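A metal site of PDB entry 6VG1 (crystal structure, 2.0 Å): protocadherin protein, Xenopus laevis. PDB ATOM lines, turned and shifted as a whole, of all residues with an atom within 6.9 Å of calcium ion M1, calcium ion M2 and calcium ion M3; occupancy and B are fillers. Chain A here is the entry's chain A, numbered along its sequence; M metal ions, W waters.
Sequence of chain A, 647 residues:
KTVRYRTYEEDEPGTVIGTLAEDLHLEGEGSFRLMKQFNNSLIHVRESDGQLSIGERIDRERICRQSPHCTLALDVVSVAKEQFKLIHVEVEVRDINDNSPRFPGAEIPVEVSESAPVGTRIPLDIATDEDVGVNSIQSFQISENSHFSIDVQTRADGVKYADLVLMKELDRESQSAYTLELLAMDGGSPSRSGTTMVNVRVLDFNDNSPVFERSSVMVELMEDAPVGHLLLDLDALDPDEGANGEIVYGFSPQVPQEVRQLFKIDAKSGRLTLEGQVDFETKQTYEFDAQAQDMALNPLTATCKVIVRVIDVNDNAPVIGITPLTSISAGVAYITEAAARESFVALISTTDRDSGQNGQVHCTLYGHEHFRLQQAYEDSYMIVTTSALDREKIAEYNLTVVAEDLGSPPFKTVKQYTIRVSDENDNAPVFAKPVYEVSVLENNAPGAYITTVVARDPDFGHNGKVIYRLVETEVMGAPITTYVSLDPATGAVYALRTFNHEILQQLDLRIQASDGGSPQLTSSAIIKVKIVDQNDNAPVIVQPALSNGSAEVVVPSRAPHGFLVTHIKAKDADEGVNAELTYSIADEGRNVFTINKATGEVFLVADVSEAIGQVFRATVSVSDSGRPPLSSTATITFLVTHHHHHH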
ATOM      1  N   GLU A 223      -9.034  17.693  34.274  1.00  0.00           N
ATOM      2  CA  GLU A 223     -10.389  17.980  34.731  1.00  0.00           C
ATOM      3  C   GLU A 223     -11.002  16.806  35.491  1.00  0.00           C
ATOM      4  O   GLU A 223     -12.066  16.965  36.108  1.00  0.00           O
ATOM      5  CB  GLU A 223     -11.312  18.374  33.571  1.00  0.00           C
ATOM      6  CG  GLU A 223     -11.683  17.324  32.582  1.00  0.00           C
ATOM      7  CD  GLU A 223     -12.859  17.743  31.691  1.00  0.00           C
ATOM      8  OE1 GLU A 223     -13.850  18.298  32.234  1.00  0.00           O
ATOM      9  OE2 GLU A 223     -12.796  17.546  30.452  1.00  0.00           O
ATOM     10  N   VAL A 278     -13.515  20.033  39.110  1.00  0.00           N
ATOM     11  CA  VAL A 278     -13.522  21.022  38.053  1.00  0.00           C
ATOM     12  C   VAL A 278     -14.113  20.376  36.804  1.00  0.00           C
ATOM     13  O   VAL A 278     -14.257  19.156  36.702  1.00  0.00           O
ATOM     14  CB  VAL A 278     -12.100  21.575  37.766  1.00  0.00           C
ATOM     15  CG1 VAL A 278     -11.578  22.351  38.949  1.00  0.00           C
ATOM     16  CG2 VAL A 278     -11.147  20.446  37.390  1.00  0.00           C
ATOM     17  N   ASP A 279     -14.480  21.214  35.831  1.00  0.00           N
ATOM     18  CA  ASP A 279     -15.091  20.723  34.601  1.00  0.00           C
ATOM     19  C   ASP A 279     -14.644  21.612  33.459  1.00  0.00           C
ATOM     20  O   ASP A 279     -15.089  22.760  33.340  1.00  0.00           O
ATOM     21  CB  ASP A 279     -16.616  20.720  34.717  1.00  0.00           C
ATOM     22  CG  ASP A 279     -17.279  20.295  33.447  1.00  0.00           C
ATOM     23  OD1 ASP A 279     -16.595  19.766  32.546  1.00  0.00           O
ATOM     24  OD2 ASP A 279     -18.519  20.489  33.336  1.00  0.00           O
ATOM     25  N   PHE A 280     -13.774  21.071  32.592  1.00  0.00           N
ATOM     26  CA  PHE A 280     -13.215  21.861  31.500  1.00  0.00           C
ATOM     27  C   PHE A 280     -14.314  22.466  30.646  1.00  0.00           C
ATOM     28  O   PHE A 280     -14.185  23.588  30.151  1.00  0.00           O
ATOM     29  CB  PHE A 280     -12.300  20.967  30.661  1.00  0.00           C
ATOM     30  CG  PHE A 280     -11.679  21.660  29.495  1.00  0.00           C
ATOM     31  CD1 PHE A 280     -10.428  22.218  29.603  1.00  0.00           C
ATOM     32  CD2 PHE A 280     -12.354  21.754  28.306  1.00  0.00           C
ATOM     33  CE1 PHE A 280      -9.850  22.862  28.533  1.00  0.00           C
ATOM     34  CE2 PHE A 280     -11.782  22.392  27.225  1.00  0.00           C
ATOM     35  CZ  PHE A 280     -10.523  22.948  27.338  1.00  0.00           C
ATOM     36  N   GLU A 281     -15.401  21.733  30.428  1.00  0.00           N
ATOM     37  CA  GLU A 281     -16.480  22.251  29.599  1.00  0.00           C
ATOM     38  C   GLU A 281     -17.242  23.393  30.245  1.00  0.00           C
ATOM     39  O   GLU A 281     -18.138  23.944  29.598  1.00  0.00           O
ATOM     40  CB  GLU A 281     -17.464  21.132  29.257  1.00  0.00           C
ATOM     41  CG  GLU A 281     -16.950  20.168  28.228  1.00  0.00           C
ATOM     42  CD  GLU A 281     -15.831  19.312  28.772  1.00  0.00           C
ATOM     43  OE1 GLU A 281     -15.882  18.933  29.978  1.00  0.00           O
ATOM     44  OE2 GLU A 281     -14.897  19.022  27.985  1.00  0.00           O
ATOM     45  N   THR A 282     -16.927  23.747  31.486  1.00  0.00           N
ATOM     46  CA  THR A 282     -17.615  24.802  32.207  1.00  0.00           C
ATOM     47  C   THR A 282     -16.706  25.986  32.486  1.00  0.00           C
ATOM     48  O   THR A 282     -17.085  27.139  32.272  1.00  0.00           O
ATOM     49  CB  THR A 282     -18.169  24.266  33.538  1.00  0.00           C
ATOM     50  OG1 THR A 282     -19.080  23.195  33.271  1.00  0.00           O
ATOM     51  CG2 THR A 282     -18.878  25.360  34.304  1.00  0.00           C
ATOM     52  N   ILE A 311      -7.293  20.936  32.003  1.00  0.00           N
ATOM     53  CA  ILE A 311      -7.005  20.196  30.779  1.00  0.00           C
ATOM     54  C   ILE A 311      -8.196  19.319  30.437  1.00  0.00           C
ATOM     55  O   ILE A 311      -8.748  18.642  31.310  1.00  0.00           O
ATOM     56  CB  ILE A 311      -5.728  19.354  30.916  1.00  0.00           C
ATOM     57  CG1 ILE A 311      -4.519  20.276  31.089  1.00  0.00           C
ATOM     58  CG2 ILE A 311      -5.582  18.444  29.722  1.00  0.00           C
ATOM     59  CD1 ILE A 311      -4.215  20.561  32.517  1.00  0.00           C
ATOM     60  N   ASP A 312      -8.548  19.279  29.157  1.00  0.00           N
ATOM     61  CA  ASP A 312      -9.769  18.615  28.728  1.00  0.00           C
ATOM     62  C   ASP A 312      -9.599  17.107  28.686  1.00  0.00           C
ATOM     63  O   ASP A 312      -8.570  16.596  28.251  1.00  0.00           O
ATOM     64  CB  ASP A 312     -10.170  19.126  27.345  1.00  0.00           C
ATOM     65  CG  ASP A 312     -11.407  18.439  26.802  1.00  0.00           C
ATOM     66  OD1 ASP A 312     -12.119  17.778  27.589  1.00  0.00           O
ATOM     67  OD2 ASP A 312     -11.662  18.564  25.577  1.00  0.00           O
ATOM     68  N   VAL A 313     -10.624  16.410  29.152  1.00  0.00           N
ATOM     69  CA  VAL A 313     -10.667  14.945  29.095  1.00  0.00           C
ATOM     70  C   VAL A 313     -11.850  14.531  28.239  1.00  0.00           C
ATOM     71  O   VAL A 313     -12.862  15.242  28.170  1.00  0.00           O
ATOM     72  CB  VAL A 313     -10.770  14.325  30.496  1.00  0.00           C
ATOM     73  CG1 VAL A 313     -10.923  12.818  30.381  1.00  0.00           C
ATOM     74  CG2 VAL A 313      -9.546  14.673  31.301  1.00  0.00           C
ATOM     75  N   ASN A 314     -11.732  13.381  27.586  1.00  0.00           N
ATOM     76  CA  ASN A 314     -12.829  12.882  26.752  1.00  0.00           C
ATOM     77  C   ASN A 314     -13.881  12.311  27.689  1.00  0.00           C
ATOM     78  O   ASN A 314     -13.996  11.097  27.892  1.00  0.00           O
ATOM     79  CB  ASN A 314     -12.366  11.860  25.739  1.00  0.00           C
ATOM     80  CG  ASN A 314     -13.389  11.651  24.644  1.00  0.00           C
ATOM     81  OD1 ASN A 314     -14.221  12.520  24.394  1.00  0.00           O
ATOM     82  ND2 ASN A 314     -13.323  10.502  23.976  1.00  0.00           N
ATOM     83  N   ASP A 315     -14.672  13.215  28.280  1.00  0.00           N
ATOM     84  CA  ASP A 315     -15.709  12.841  29.221  1.00  0.00           C
ATOM     85  C   ASP A 315     -17.109  13.138  28.680  1.00  0.00           C
ATOM     86  O   ASP A 315     -18.081  13.143  29.443  1.00  0.00           O
ATOM     87  CB  ASP A 315     -15.494  13.534  30.564  1.00  0.00           C
ATOM     88  CG  ASP A 315     -15.472  15.056  30.459  1.00  0.00           C
ATOM     89  OD1 ASP A 315     -15.236  15.606  29.361  1.00  0.00           O
ATOM     90  OD2 ASP A 315     -15.687  15.691  31.498  1.00  0.00           O
ATOM     91  N   ASN A 316     -17.221  13.348  27.370  1.00  0.00           N
ATOM     92  CA  ASN A 316     -18.520  13.499  26.731  1.00  0.00           C
ATOM     93  C   ASN A 316     -18.562  12.666  25.461  1.00  0.00           C
ATOM     94  O   ASN A 316     -17.561  12.544  24.753  1.00  0.00           O
ATOM     95  CB  ASN A 316     -18.824  14.962  26.370  1.00  0.00           C
ATOM     96  CG  ASN A 316     -19.142  15.808  27.591  1.00  0.00           C
ATOM     97  OD1 ASN A 316     -20.307  15.915  28.006  1.00  0.00           O
ATOM     98  ND2 ASN A 316     -18.113  16.390  28.175  1.00  0.00           N
ATOM     99  N   ALA A 317     -19.731  12.118  25.164  1.00  0.00           N
ATOM    100  CA  ALA A 317     -19.961  11.390  23.938  1.00  0.00           C
ATOM    101  C   ALA A 317     -20.733  12.250  22.964  1.00  0.00           C
ATOM    102  O   ALA A 317     -21.312  13.263  23.346  1.00  0.00           O
ATOM    103  CB  ALA A 317     -20.732  10.100  24.212  1.00  0.00           C
ATOM    104  N   PRO A 318     -20.736  11.887  21.681  1.00  0.00           N
ATOM    105  CA  PRO A 318     -21.543  12.647  20.717  1.00  0.00           C
ATOM    106  C   PRO A 318     -23.027  12.604  21.029  1.00  0.00           C
ATOM    107  O   PRO A 318     -23.559  11.591  21.503  1.00  0.00           O
ATOM    108  CB  PRO A 318     -21.237  11.962  19.381  1.00  0.00           C
ATOM    109  CG  PRO A 318     -19.853  11.402  19.585  1.00  0.00           C
ATOM    110  CD  PRO A 318     -19.785  10.968  21.031  1.00  0.00           C
ATOM    111  N   ASP A 352     -20.238  17.289  20.242  1.00  0.00           N
ATOM    112  CA  ASP A 352     -19.437  16.706  21.322  1.00  0.00           C
ATOM    113  C   ASP A 352     -18.970  17.855  22.194  1.00  0.00           C
ATOM    114  O   ASP A 352     -18.307  18.767  21.707  1.00  0.00           O
ATOM    115  CB  ASP A 352     -18.235  15.922  20.779  1.00  0.00           C
ATOM    116  CG  ASP A 352     -17.591  15.001  21.824  1.00  0.00           C
ATOM    117  OD1 ASP A 352     -17.606  13.765  21.619  1.00  0.00           O
ATOM    118  OD2 ASP A 352     -17.038  15.507  22.836  1.00  0.00           O
ATOM    119  N   ARG A 353     -19.320  17.825  23.487  1.00  0.00           N
ATOM    120  CA  ARG A 353     -19.021  18.945  24.373  1.00  0.00           C
ATOM    121  C   ARG A 353     -17.517  19.168  24.539  1.00  0.00           C
ATOM    122  O   ARG A 353     -17.111  20.262  24.953  1.00  0.00           O
ATOM    123  CB  ARG A 353     -19.596  18.716  25.786  1.00  0.00           C
ATOM    124  CG  ARG A 353     -21.092  18.480  25.857  1.00  0.00           C
ATOM    125  CD  ARG A 353     -21.832  19.808  25.877  1.00  0.00           C
ATOM    126  NE  ARG A 353     -21.529  20.593  27.074  1.00  0.00           N
ATOM    127  CZ  ARG A 353     -21.898  21.849  27.231  1.00  0.00           C
ATOM    128  NH1 ARG A 353     -22.569  22.456  26.261  1.00  0.00           N
ATOM    129  NH2 ARG A 353     -21.593  22.511  28.341  1.00  0.00           N
ATOM    130  N   ASP A 354     -16.702  18.141  24.315  1.00  0.00           N
ATOM    131  CA  ASP A 354     -15.277  18.281  24.563  1.00  0.00           C
ATOM    132  C   ASP A 354     -14.627  19.155  23.483  1.00  0.00           C
ATOM    133  O   ASP A 354     -15.280  19.701  22.589  1.00  0.00           O
ATOM    134  CB  ASP A 354     -14.591  16.913  24.588  1.00  0.00           C
ATOM    135  CG  ASP A 354     -15.216  15.976  25.589  1.00  0.00           C
ATOM    136  OD1 ASP A 354     -15.353  16.364  26.778  1.00  0.00           O
ATOM    137  OD2 ASP A 354     -15.568  14.844  25.191  1.00  0.00           O
ATOM    138  N   SER A 355     -13.303  19.251  23.551  1.00  0.00           N
ATOM    139  CA  SER A 355     -12.497  20.047  22.629  1.00  0.00           C
ATOM    140  C   SER A 355     -11.407  19.189  22.000  1.00  0.00           C
ATOM    141  O   SER A 355     -11.112  18.074  22.443  1.00  0.00           O
ATOM    142  CB  SER A 355     -11.867  21.242  23.354  1.00  0.00           C
ATOM    143  OG  SER A 355     -12.868  22.116  23.822  1.00  0.00           O
ATOM    144  N   GLN A 357      -9.502  16.772  19.287  1.00  0.00           N
ATOM    145  CA  GLN A 357      -9.955  15.500  18.725  1.00  0.00           C
ATOM    146  C   GLN A 357     -11.076  14.894  19.550  1.00  0.00           C
ATOM    147  O   GLN A 357     -11.973  14.242  18.997  1.00  0.00           O
ATOM    148  CB  GLN A 357      -8.787  14.519  18.658  1.00  0.00           C
ATOM    149  CG  GLN A 357      -7.647  14.930  17.747  1.00  0.00           C
ATOM    150  CD  GLN A 357      -7.852  14.496  16.313  1.00  0.00           C
ATOM    151  OE1 GLN A 357      -8.195  13.344  16.038  1.00  0.00           O
ATOM    152  NE2 GLN A 357      -7.665  15.423  15.383  1.00  0.00           N
ATOM    153  N   ASN A 358     -11.042  15.094  20.866  1.00  0.00           N
ATOM    154  CA  ASN A 358     -12.058  14.509  21.726  1.00  0.00           C
ATOM    155  C   ASN A 358     -13.436  15.085  21.428  1.00  0.00           C
ATOM    156  O   ASN A 358     -14.440  14.426  21.736  1.00  0.00           O
ATOM    157  CB  ASN A 358     -11.700  14.727  23.196  1.00  0.00           C
ATOM    158  CG  ASN A 358     -10.435  13.997  23.596  1.00  0.00           C
ATOM    159  OD1 ASN A 358     -10.094  12.968  23.028  1.00  0.00           O
ATOM    160  ND2 ASN A 358      -9.766  14.505  24.620  1.00  0.00           N
ATOM    161  N   GLY A 359     -13.508  16.272  20.818  1.00  0.00           N
ATOM    162  CA  GLY A 359     -14.774  16.895  20.502  1.00  0.00           C
ATOM    163  C   GLY A 359     -15.132  16.907  19.037  1.00  0.00           C
ATOM    164  O   GLY A 359     -16.120  17.536  18.663  1.00  0.00           O
ATOM    165  N   GLN A 360     -14.362  16.235  18.190  1.00  0.00           N
ATOM    166  CA  GLN A 360     -14.548  16.261  16.751  1.00  0.00           C
ATOM    167  C   GLN A 360     -15.312  15.019  16.346  1.00  0.00           C
ATOM    168  O   GLN A 360     -14.919  13.898  16.698  1.00  0.00           O
ATOM    169  CB  GLN A 360     -13.185  16.310  16.074  1.00  0.00           C
ATOM    170  CG  GLN A 360     -13.214  16.703  14.645  1.00  0.00           C
ATOM    171  CD  GLN A 360     -11.833  17.142  14.190  1.00  0.00           C
ATOM    172  OE1 GLN A 360     -11.188  17.966  14.835  1.00  0.00           O
ATOM    173  NE2 GLN A 360     -11.372  16.591  13.080  1.00  0.00           N
ATOM    174  N   VAL A 361     -16.399  15.202  15.592  1.00  0.00           N
ATOM    175  CA  VAL A 361     -17.353  14.130  15.334  1.00  0.00           C
ATOM    176  C   VAL A 361     -17.355  13.749  13.861  1.00  0.00           C
ATOM    177  O   VAL A 361     -17.339  14.614  12.975  1.00  0.00           O
ATOM    178  CB  VAL A 361     -18.776  14.518  15.767  1.00  0.00           C
ATOM    179  CG1 VAL A 361     -18.813  14.844  17.238  1.00  0.00           C
ATOM    180  CG2 VAL A 361     -19.281  15.710  14.938  1.00  0.00           C
ATOM    181  N   ASP A 405     -16.541  10.308  18.040  1.00  0.00           N
ATOM    182  CA  ASP A 405     -15.541  11.355  18.222  1.00  0.00           C
ATOM    183  C   ASP A 405     -14.161  10.764  17.913  1.00  0.00           C
ATOM    184  O   ASP A 405     -14.021   9.565  17.625  1.00  0.00           O
ATOM    185  CB  ASP A 405     -15.627  11.982  19.632  1.00  0.00           C
ATOM    186  CG  ASP A 405     -15.085  11.103  20.733  1.00  0.00           C
ATOM    187  OD1 ASP A 405     -14.489  10.036  20.432  1.00  0.00           O
ATOM    188  OD2 ASP A 405     -15.271  11.484  21.918  1.00  0.00           O
ATOM    189  N   LEU A 406     -13.128  11.601  17.963  1.00  0.00           N
ATOM    190  CA  LEU A 406     -11.779  11.174  17.621  1.00  0.00           C
ATOM    191  C   LEU A 406     -10.911  11.008  18.862  1.00  0.00           C
ATOM    192  O   LEU A 406      -9.690  11.144  18.789  1.00  0.00           O
ATOM    193  CB  LEU A 406     -11.146  12.146  16.641  1.00  0.00           C
ATOM    194  CG  LEU A 406     -11.453  11.927  15.170  1.00  0.00           C
ATOM    195  CD1 LEU A 406     -10.760  10.644  14.676  1.00  0.00           C
ATOM    196  CD2 LEU A 406     -12.949  11.836  14.865  1.00  0.00           C
ATOM    197  N   GLY A 407     -11.519  10.672  19.992  1.00  0.00           N
ATOM    198  CA  GLY A 407     -10.757  10.351  21.180  1.00  0.00           C
ATOM    199  C   GLY A 407     -10.049   9.013  21.040  1.00  0.00           C
ATOM    200  O   GLY A 407     -10.212   8.270  20.090  1.00  0.00           O
ATOM    201  N   PHE A 411     -15.647   7.692  21.712  1.00  0.00           N
ATOM    202  CA  PHE A 411     -17.049   7.485  22.073  1.00  0.00           C
ATOM    203  C   PHE A 411     -17.850   7.317  20.799  1.00  0.00           C
ATOM    204  O   PHE A 411     -17.624   8.030  19.817  1.00  0.00           O
ATOM    205  CB  PHE A 411     -17.595   8.671  22.875  1.00  0.00           C
ATOM    206  CG  PHE A 411     -17.426   8.542  24.388  1.00  0.00           C
ATOM    207  CD1 PHE A 411     -18.194   7.628  25.099  1.00  0.00           C
ATOM    208  CD2 PHE A 411     -16.521   9.346  25.080  1.00  0.00           C
ATOM    209  CE1 PHE A 411     -18.042   7.513  26.478  1.00  0.00           C
ATOM    210  CE2 PHE A 411     -16.376   9.224  26.431  1.00  0.00           C
ATOM    211  CZ  PHE A 411     -17.131   8.322  27.147  1.00  0.00           C
HETATM  212 CA    CA M   1     -16.163  17.646  31.931  1.00  0.00          CA
HETATM  213 CA    CA M   2     -13.995  17.187  28.485  1.00  0.00          CA
HETATM  214 CA    CA M   3     -15.915  13.463  23.184  1.00  0.00          CA
HETATM  215  O   HOH W   1     -18.338  17.151  31.327  1.00  0.00           O
HETATM  216  O   HOH W   2     -16.813  17.229  34.210  1.00  0.00           O
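O of Asn 358 binds calcium ion M3 (2.3 Å). Calcium ion M3 is bound by OD1 of Asn 314, 2.3 Å away. Calcium ion M3 is bound by the side-chain carboxylate (OD1) of Asp 352, 2.3 Å away. OD2 of Asp 352 is bound to calcium ion M3 (2.4 Å). Calcium ion M3 is bound by the side-chain carboxylate (OD2) of Asp 405 (2.4 Å). O of Asn 316 binds calcium ion M3 (2.5 Å). The side-chain carboxylate (OD2) of Asp 354 is bound to calcium ion M3, 2.5 Å away.
Six residues have an atom within 4 Å of calcium ion M3: Asn 314, Asn 316, Asp 352, Asp 354, Asn 358 and Asp 405. The nearest printed residue that does not touch calcium ion M3 is Gly 359 (4.4 Å).
OD2 of Asp 315 binds calcium ion M1, at 2.1 Å. OD1 of Asp 279 is bound to calcium ion M1. Water W1 binds calcium ion M1, at 2.3 Å. Calcium ion M1 is bound by the side-chain carboxylate (OE1) of Glu 281. Water W2 binds calcium ion M1, 2.4 Å away. OE1 of Glu 223 is bound to calcium ion M1 (2.4 Å). Calcium ion M1 has six donor atoms within binding distance.
Four residues have an atom within 4 Å of calcium ion M1: Glu 223, Asp 279, Glu 281 and Asp 315.
Calcium ion M2 is bound by the side-chain carboxylate (OE2) of Glu 281, the side-chain carboxylate (OD1) of Asp 312, the side-chain carboxylate (OD1) of Asp 315, the backbone carbonyl oxygen (O) of Val 313, the side-chain carboxylate (OD1) of Asp 354 and the side-chain carboxylate (OE2) of Glu 223. Slightly farther from calcium ion M2 lies OE1 of Glu 281 (3.0 Å).
Of the 27 residues printed, 6 come within 4 Å of calcium ion M2.
ND2 of Asn 316 lies close to OD1 of Asp 315, at 3.2 Å. The side-chain carboxylate (OD2) of Asp 312 lies within hydrogen-bond range of the backbone NH (N) of Ser 355 (2.7 Å). The side-chain carboxylate (OD2) of Asp 279 is in hydrogen-bond range of the side-chain hydroxyl (OG1) of Thr 282, 2.8 Å away. N of Phe 280 lies close to OE1 of Glu 223 (2.8 Å). The backbone NH (N) of Glu 223 sits at hydrogen-bond distance from the backbone carbonyl oxygen (O) of Ile 311 (3.1 Å). The backbone NH (N) of Phe 411 is in hydrogen-bond range of the side-chain carboxylate (OD1) of Asp 405 (2.9 Å). The backbone NH of Gly 407 lies within hydrogen-bond range of the side-chain carboxylate of Asp 405, 3.1 Å away.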
